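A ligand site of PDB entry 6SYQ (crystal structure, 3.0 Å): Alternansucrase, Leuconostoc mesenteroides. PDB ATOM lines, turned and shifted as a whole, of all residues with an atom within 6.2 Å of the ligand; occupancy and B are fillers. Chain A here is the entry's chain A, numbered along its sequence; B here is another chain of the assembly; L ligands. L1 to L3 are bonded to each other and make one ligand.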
ATOM      1  N   TYR A 546     -29.154 -14.842   8.038  1.00  0.00           N
ATOM      2  CA  TYR A 546     -30.202 -13.846   8.110  1.00  0.00           C
ATOM      3  C   TYR A 546     -29.638 -12.446   8.287  1.00  0.00           C
ATOM      4  O   TYR A 546     -30.280 -11.476   7.886  1.00  0.00           O
ATOM      5  CB  TYR A 546     -31.244 -14.181   9.205  1.00  0.00           C
ATOM      6  CG  TYR A 546     -32.475 -13.316   9.080  1.00  0.00           C
ATOM      7  CD1 TYR A 546     -33.187 -13.291   7.888  1.00  0.00           C
ATOM      8  CD2 TYR A 546     -32.879 -12.488  10.110  1.00  0.00           C
ATOM      9  CE1 TYR A 546     -34.287 -12.471   7.725  1.00  0.00           C
ATOM     10  CE2 TYR A 546     -33.977 -11.664   9.954  1.00  0.00           C
ATOM     11  CZ  TYR A 546     -34.678 -11.660   8.757  1.00  0.00           C
ATOM     12  OH  TYR A 546     -35.788 -10.868   8.541  1.00  0.00           O
ATOM     13  N   THR A 547     -28.447 -12.318   8.837  1.00  0.00           N
ATOM     14  CA  THR A 547     -27.908 -11.001   9.167  1.00  0.00           C
ATOM     15  C   THR A 547     -27.753 -10.174   7.901  1.00  0.00           C
ATOM     16  O   THR A 547     -28.024  -8.980   7.898  1.00  0.00           O
ATOM     17  CB  THR A 547     -26.573 -11.060   9.925  1.00  0.00           C
ATOM     18  OG1 THR A 547     -25.574 -11.647   9.100  1.00  0.00           O
ATOM     19  CG2 THR A 547     -26.701 -11.884  11.215  1.00  0.00           C
ATOM     20  N   VAL A 548     -27.358 -10.810   6.808  1.00  0.00           N
ATOM     21  CA  VAL A 548     -27.243 -10.099   5.530  1.00  0.00           C
ATOM     22  C   VAL A 548     -28.616  -9.911   4.830  1.00  0.00           C
ATOM     23  O   VAL A 548     -28.900  -8.853   4.280  1.00  0.00           O
ATOM     24  CB  VAL A 548     -26.203 -10.735   4.596  1.00  0.00           C
ATOM     25  CG1 VAL A 548     -26.678 -12.083   4.083  1.00  0.00           C
ATOM     26  CG2 VAL A 548     -25.911  -9.821   3.425  1.00  0.00           C
ATOM     27  N   SER A 550     -31.427  -9.597   6.318  1.00  0.00           N
ATOM     28  CA  SER A 550     -31.998  -8.564   7.151  1.00  0.00           C
ATOM     29  C   SER A 550     -31.542  -7.164   6.729  1.00  0.00           C
ATOM     30  O   SER A 550     -32.368  -6.254   6.562  1.00  0.00           O
ATOM     31  CB  SER A 550     -31.608  -8.809   8.609  1.00  0.00           C
ATOM     32  OG  SER A 550     -31.880  -7.728   9.450  1.00  0.00           O
ATOM     33  N   GLN A 551     -30.240  -6.994   6.521  1.00  0.00           N
ATOM     34  CA  GLN A 551     -29.715  -5.704   6.195  1.00  0.00           C
ATOM     35  C   GLN A 551     -30.142  -5.281   4.795  1.00  0.00           C
ATOM     36  O   GLN A 551     -30.252  -4.091   4.539  1.00  0.00           O
ATOM     37  CB  GLN A 551     -28.205  -5.744   6.264  1.00  0.00           C
ATOM     38  CG  GLN A 551     -27.555  -4.382   6.381  1.00  0.00           C
ATOM     39  CD  GLN A 551     -27.946  -3.719   7.680  1.00  0.00           C
ATOM     40  OE1 GLN A 551     -27.687  -4.234   8.754  1.00  0.00           O
ATOM     41  NE2 GLN A 551     -28.613  -2.605   7.570  1.00  0.00           N
ATOM     42  N   ASN A 554     -33.413  -3.544   5.326  1.00  0.00           N
ATOM     43  CA  ASN A 554     -33.359  -2.247   5.959  1.00  0.00           C
ATOM     44  C   ASN A 554     -32.770  -1.183   5.098  1.00  0.00           C
ATOM     45  O   ASN A 554     -33.231  -0.035   5.128  1.00  0.00           O
ATOM     46  CB  ASN A 554     -32.536  -2.319   7.236  1.00  0.00           C
ATOM     47  CG  ASN A 554     -33.148  -3.249   8.275  1.00  0.00           C
ATOM     48  OD1 ASN A 554     -32.471  -3.667   9.197  1.00  0.00           O
ATOM     49  ND2 ASN A 554     -34.438  -3.534   8.148  1.00  0.00           N
ATOM     50  N   SER A 555     -31.725  -1.548   4.338  1.00  0.00           N
ATOM     51  CA  SER A 555     -30.961  -0.584   3.564  1.00  0.00           C
ATOM     52  C   SER A 555     -31.349  -0.454   2.066  1.00  0.00           C
ATOM     53  O   SER A 555     -31.019   0.554   1.453  1.00  0.00           O
ATOM     54  CB  SER A 555     -29.480  -0.907   3.683  1.00  0.00           C
ATOM     55  OG  SER A 555     -29.032  -0.825   5.038  1.00  0.00           O
ATOM     56  N   SER A 564     -32.064   2.273   6.336  1.00  0.00           N
ATOM     57  CA  SER A 564     -30.820   2.350   7.064  1.00  0.00           C
ATOM     58  C   SER A 564     -29.723   2.622   6.048  1.00  0.00           C
ATOM     59  O   SER A 564     -29.810   2.185   4.889  1.00  0.00           O
ATOM     60  CB  SER A 564     -30.550   1.050   7.802  1.00  0.00           C
ATOM     61  OG  SER A 564     -31.682   0.651   8.529  1.00  0.00           O
ATOM     62  N   ASN A 565     -28.686   3.330   6.467  1.00  0.00           N
ATOM     63  CA  ASN A 565     -27.565   3.573   5.583  1.00  0.00           C
ATOM     64  C   ASN A 565     -26.846   2.298   5.133  1.00  0.00           C
ATOM     65  O   ASN A 565     -26.853   1.259   5.827  1.00  0.00           O
ATOM     66  CB  ASN A 565     -26.562   4.482   6.257  1.00  0.00           C
ATOM     67  CG  ASN A 565     -27.001   5.894   6.261  1.00  0.00           C
ATOM     68  OD1 ASN A 565     -28.103   6.212   5.820  1.00  0.00           O
ATOM     69  ND2 ASN A 565     -26.142   6.773   6.724  1.00  0.00           N
ATOM     70  N   TRP A 567     -23.802   2.098   5.157  1.00  0.00           N
ATOM     71  CA  TRP A 567     -22.816   1.928   6.234  1.00  0.00           C
ATOM     72  C   TRP A 567     -23.060   0.680   7.089  1.00  0.00           C
ATOM     73  O   TRP A 567     -22.116   0.024   7.501  1.00  0.00           O
ATOM     74  CB  TRP A 567     -22.849   3.143   7.157  1.00  0.00           C
ATOM     75  CG  TRP A 567     -21.784   3.173   8.206  1.00  0.00           C
ATOM     76  CD1 TRP A 567     -20.461   3.444   8.013  1.00  0.00           C
ATOM     77  CD2 TRP A 567     -21.957   2.949   9.616  1.00  0.00           C
ATOM     78  NE1 TRP A 567     -19.787   3.385   9.223  1.00  0.00           N
ATOM     79  CE2 TRP A 567     -20.678   3.081  10.214  1.00  0.00           C
ATOM     80  CE3 TRP A 567     -23.057   2.635  10.421  1.00  0.00           C
ATOM     81  CZ2 TRP A 567     -20.481   2.924  11.573  1.00  0.00           C
ATOM     82  CZ3 TRP A 567     -22.863   2.475  11.772  1.00  0.00           C
ATOM     83  CH2 TRP A 567     -21.582   2.638  12.342  1.00  0.00           C
ATOM     84  N   TYR A 568     -24.311   0.360   7.336  1.00  0.00           N
ATOM     85  CA  TYR A 568     -24.650  -0.808   8.189  1.00  0.00           C
ATOM     86  C   TYR A 568     -24.192  -2.163   7.627  1.00  0.00           C
ATOM     87  O   TYR A 568     -23.963  -3.092   8.382  1.00  0.00           O
ATOM     88  CB  TYR A 568     -26.151  -0.826   8.537  1.00  0.00           C
ATOM     89  CG  TYR A 568     -26.478   0.239   9.556  1.00  0.00           C
ATOM     90  CD1 TYR A 568     -26.105   0.076  10.890  1.00  0.00           C
ATOM     91  CD2 TYR A 568     -27.116   1.422   9.194  1.00  0.00           C
ATOM     92  CE1 TYR A 568     -26.380   1.040  11.844  1.00  0.00           C
ATOM     93  CE2 TYR A 568     -27.388   2.394  10.144  1.00  0.00           C
ATOM     94  CZ  TYR A 568     -27.017   2.186  11.464  1.00  0.00           C
ATOM     95  OH  TYR A 568     -27.248   3.122  12.427  1.00  0.00           O
ATOM     96  N   PHE A 569     -24.009  -2.241   6.307  1.00  0.00           N
ATOM     97  CA  PHE A 569     -23.458  -3.430   5.693  1.00  0.00           C
ATOM     98  C   PHE A 569     -22.032  -3.739   6.139  1.00  0.00           C
ATOM     99  O   PHE A 569     -21.616  -4.888   6.114  1.00  0.00           O
ATOM    100  CB  PHE A 569     -23.483  -3.339   4.173  1.00  0.00           C
ATOM    101  CG  PHE A 569     -24.826  -3.593   3.574  1.00  0.00           C
ATOM    102  CD1 PHE A 569     -25.335  -4.872   3.507  1.00  0.00           C
ATOM    103  CD2 PHE A 569     -25.561  -2.557   3.049  1.00  0.00           C
ATOM    104  CE1 PHE A 569     -26.572  -5.104   2.940  1.00  0.00           C
ATOM    105  CE2 PHE A 569     -26.791  -2.777   2.486  1.00  0.00           C
ATOM    106  CZ  PHE A 569     -27.310  -4.056   2.433  1.00  0.00           C
ATOM    107  N   LEU A 570     -21.271  -2.732   6.555  1.00  0.00           N
ATOM    108  CA  LEU A 570     -19.891  -2.965   6.947  1.00  0.00           C
ATOM    109  C   LEU A 570     -19.752  -3.662   8.289  1.00  0.00           C
ATOM    110  O   LEU A 570     -18.854  -4.478   8.455  1.00  0.00           O
ATOM    111  CB  LEU A 570     -19.122  -1.661   6.978  1.00  0.00           C
ATOM    112  CG  LEU A 570     -19.129  -0.873   5.673  1.00  0.00           C
ATOM    113  CD1 LEU A 570     -18.316   0.402   5.829  1.00  0.00           C
ATOM    114  CD2 LEU A 570     -18.589  -1.691   4.496  1.00  0.00           C
ATOM    115  N   ASP A 571     -20.630  -3.350   9.244  1.00  0.00           N
ATOM    116  CA  ASP A 571     -20.502  -3.817  10.623  1.00  0.00           C
ATOM    117  C   ASP A 571     -19.108  -3.472  11.160  1.00  0.00           C
ATOM    118  O   ASP A 571     -18.306  -4.355  11.474  1.00  0.00           O
ATOM    119  CB  ASP A 571     -20.815  -5.319  10.703  1.00  0.00           C
ATOM    120  CG  ASP A 571     -20.780  -5.865  12.129  1.00  0.00           C
ATOM    121  OD1 ASP A 571     -21.086  -5.113  13.088  1.00  0.00           O
ATOM    122  OD2 ASP A 571     -20.417  -7.047  12.278  1.00  0.00           O
ATOM    123  N   THR A 572     -18.818  -2.184  11.246  1.00  0.00           N
ATOM    124  CA  THR A 572     -17.470  -1.727  11.667  1.00  0.00           C
ATOM    125  C   THR A 572     -17.122  -2.133  13.099  1.00  0.00           C
ATOM    126  O   THR A 572     -15.952  -2.301  13.445  1.00  0.00           O
ATOM    127  CB  THR A 572     -17.342  -0.195  11.524  1.00  0.00           C
ATOM    128  OG1 THR A 572     -18.424   0.445  12.192  1.00  0.00           O
ATOM    129  CG2 THR A 572     -17.367   0.208  10.056  1.00  0.00           C
ATOM    130  N   ARG A 589     -17.854  -9.020  22.201  1.00  0.00           N
ATOM    131  CA  ARG A 589     -18.888  -8.113  21.740  1.00  0.00           C
ATOM    132  C   ARG A 589     -20.212  -8.494  22.402  1.00  0.00           C
ATOM    133  O   ARG A 589     -20.359  -9.621  22.875  1.00  0.00           O
ATOM    134  CB  ARG A 589     -19.015  -8.261  20.229  1.00  0.00           C
ATOM    135  CG  ARG A 589     -17.856  -7.688  19.434  1.00  0.00           C
ATOM    136  CD  ARG A 589     -18.203  -7.676  17.940  1.00  0.00           C
ATOM    137  NE  ARG A 589     -19.250  -6.697  17.625  1.00  0.00           N
ATOM    138  CZ  ARG A 589     -19.795  -6.502  16.421  1.00  0.00           C
ATOM    139  NH1 ARG A 589     -19.419  -7.207  15.367  1.00  0.00           N
ATOM    140  NH2 ARG A 589     -20.720  -5.570  16.280  1.00  0.00           N
ATOM    141  N   SER A 592     -23.740  -9.293  18.814  1.00  0.00           N
ATOM    142  CA  SER A 592     -24.227  -8.508  17.686  1.00  0.00           C
ATOM    143  C   SER A 592     -23.318  -8.612  16.461  1.00  0.00           C
ATOM    144  O   SER A 592     -22.159  -9.019  16.539  1.00  0.00           O
ATOM    145  CB  SER A 592     -24.336  -7.041  18.114  1.00  0.00           C
ATOM    146  OG  SER A 592     -23.247  -6.634  18.955  1.00  0.00           O
ATOM    147  N   GLY A 593     -23.880  -8.227  15.326  1.00  0.00           N
ATOM    148  CA  GLY A 593     -23.088  -8.059  14.109  1.00  0.00           C
ATOM    149  C   GLY A 593     -23.362  -9.089  13.038  1.00  0.00           C
ATOM    150  O   GLY A 593     -24.040 -10.089  13.275  1.00  0.00           O
ATOM    151  N   THR A 594     -22.851  -8.809  11.838  1.00  0.00           N
ATOM    152  CA  THR A 594     -23.083  -9.651  10.676  1.00  0.00           C
ATOM    153  C   THR A 594     -22.177 -10.856  10.811  1.00  0.00           C
ATOM    154  O   THR A 594     -21.100 -10.758  11.394  1.00  0.00           O
ATOM    155  CB  THR A 594     -22.839  -8.862   9.372  1.00  0.00           C
ATOM    156  OG1 THR A 594     -23.643  -9.386   8.306  1.00  0.00           O
ATOM    157  CG2 THR A 594     -21.362  -8.839   8.995  1.00  0.00           C
ATOM    158  N   ASN B 101     -38.037   7.587  13.724  1.00  0.00           N
ATOM    159  CA  ASN B 101     -37.910   6.586  14.793  1.00  0.00           C
ATOM    160  C   ASN B 101     -39.161   6.403  15.661  1.00  0.00           C
ATOM    161  O   ASN B 101     -39.111   5.720  16.680  1.00  0.00           O
ATOM    162  CB  ASN B 101     -36.685   6.899  15.663  1.00  0.00           C
ATOM    163  CG  ASN B 101     -35.397   6.525  14.981  1.00  0.00           C
ATOM    164  OD1 ASN B 101     -35.178   5.355  14.643  1.00  0.00           O
ATOM    165  ND2 ASN B 101     -34.536   7.506  14.744  1.00  0.00           N
HETATM  166  C1  LIG L   1     -32.801  -3.262  16.740  1.00  0.00           C
HETATM  167  C2  LIG L   1     -34.198  -2.619  16.767  1.00  0.00           C
HETATM  168  C3  LIG L   1     -34.531  -2.042  15.378  1.00  0.00           C
HETATM  169  C4  LIG L   1     -33.452  -1.030  15.024  1.00  0.00           C
HETATM  170  C5  LIG L   1     -32.079  -1.699  15.099  1.00  0.00           C
HETATM  171  C6  LIG L   1     -30.976  -0.680  14.814  1.00  0.00           C
HETATM  172  O1  LIG L   1     -32.703  -4.305  15.795  1.00  0.00           O
HETATM  173  O2  LIG L   1     -35.164  -3.521  17.296  1.00  0.00           O
HETATM  174  O3  LIG L   1     -35.769  -1.380  15.327  1.00  0.00           O
HETATM  175  O4  LIG L   1     -33.664  -0.483  13.732  1.00  0.00           O
HETATM  176  O5  LIG L   1     -31.865  -2.262  16.386  1.00  0.00           O
HETATM  177  O6  LIG L   1     -30.972  -0.438  13.434  1.00  0.00           O
HETATM  178  C1  LG2 L   2     -29.606  -0.611  12.805  1.00  0.00           C
HETATM  179  C2  LG2 L   2     -29.706  -0.667  11.299  1.00  0.00           C
HETATM  180  C3  LG2 L   2     -30.343  -2.008  10.923  1.00  0.00           C
HETATM  181  C4  LG2 L   2     -29.429  -3.095  11.454  1.00  0.00           C
HETATM  182  C5  LG2 L   2     -29.328  -2.978  12.978  1.00  0.00           C
HETATM  183  C6  LG2 L   2     -28.336  -4.020  13.494  1.00  0.00           C
HETATM  184  O1  LG2 L   2     -30.532   0.392  10.866  1.00  0.00           O
HETATM  185  O2  LG2 L   2     -30.412  -2.137   9.522  1.00  0.00           O
HETATM  186  O3  LG2 L   2     -29.859  -4.382  11.048  1.00  0.00           O
HETATM  187  O4  LG2 L   2     -28.854  -1.681  13.329  1.00  0.00           O
HETATM  188  O5  LG2 L   2     -27.049  -3.652  13.049  1.00  0.00           O
HETATM  189  C1  LG3 L   3     -26.077  -4.680  13.333  1.00  0.00           C
HETATM  190  C2  LG3 L   3     -24.728  -4.238  12.807  1.00  0.00           C
HETATM  191  C3  LG3 L   3     -24.889  -3.938  11.321  1.00  0.00           C
HETATM  192  C4  LG3 L   3     -25.272  -5.244  10.639  1.00  0.00           C
HETATM  193  C5  LG3 L   3     -26.524  -5.857  11.301  1.00  0.00           C
HETATM  194  C6  LG3 L   3     -26.709  -7.291  10.838  1.00  0.00           C
HETATM  195  O1  LG3 L   3     -24.302  -3.086  13.476  1.00  0.00           O
HETATM  196  O2  LG3 L   3     -23.674  -3.414  10.830  1.00  0.00           O
HETATM  197  O3  LG3 L   3     -25.468  -5.059   9.265  1.00  0.00           O
HETATM  198  O4  LG3 L   3     -26.429  -5.897  12.714  1.00  0.00           O
HETATM  199  O5  LG3 L   3     -27.802  -7.861  11.503  1.00  0.00           O
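The side-chain amide oxygen (OE1) of Gln 551 sits at hydrogen-bond distance from an oxygen (O3) of LG3 L3.
O2 of LG3 L3 lies within hydrogen-bond range of O of Tyr 568 (2.5 Å).
An oxygen (O2) of LG2 L2 is in hydrogen-bond range of the side-chain amide oxygen of Asn 554, 2.6 Å away.
OG of Ser 564 is in hydrogen-bond range of O1 of LG2 L2, at 2.6 Å.
N of Asp 571 lies close to O2 of LG3 L3 (3.4 Å).
The side-chain amide nitrogen of Gln 551 lies within hydrogen-bond range of the side-chain hydroxyl of Ser 555 (3.1 Å).
The backbone carbonyl oxygen (O) of Asn 554 sits at hydrogen-bond distance from the backbone NH (N) of Ser 564.
The backbone carbonyl oxygen (O) of Ser 564 sits at hydrogen-bond distance from the side-chain hydroxyl (OG) of Ser 555 (3.1 Å).
The backbone NH (N) of Thr 594 lies within hydrogen-bond range of the side-chain carboxylate (OD2) of Asp 571, at 3.0 Å.
NH2 of Arg 589 lies within salt-bridge range of OD1 of Asp 571 (3.2 Å).
The side-chain hydroxyl (OG1) of Thr 547 sits at hydrogen-bond distance from the side-chain hydroxyl (OG1) of Thr 594 (3.1 Å).
Residues that only touch the ligand: Thr 547.
Hydrophobic or aromatic side chains that line the ligand: Tyr 568.
Within 4 Å of the ligand: Thr 547, Gln 551, Asn 554, Ser 564, Tyr 568 and Asp 571.
The nearest printed residue that does not touch the ligand is Gly 593 (4.2 Å).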
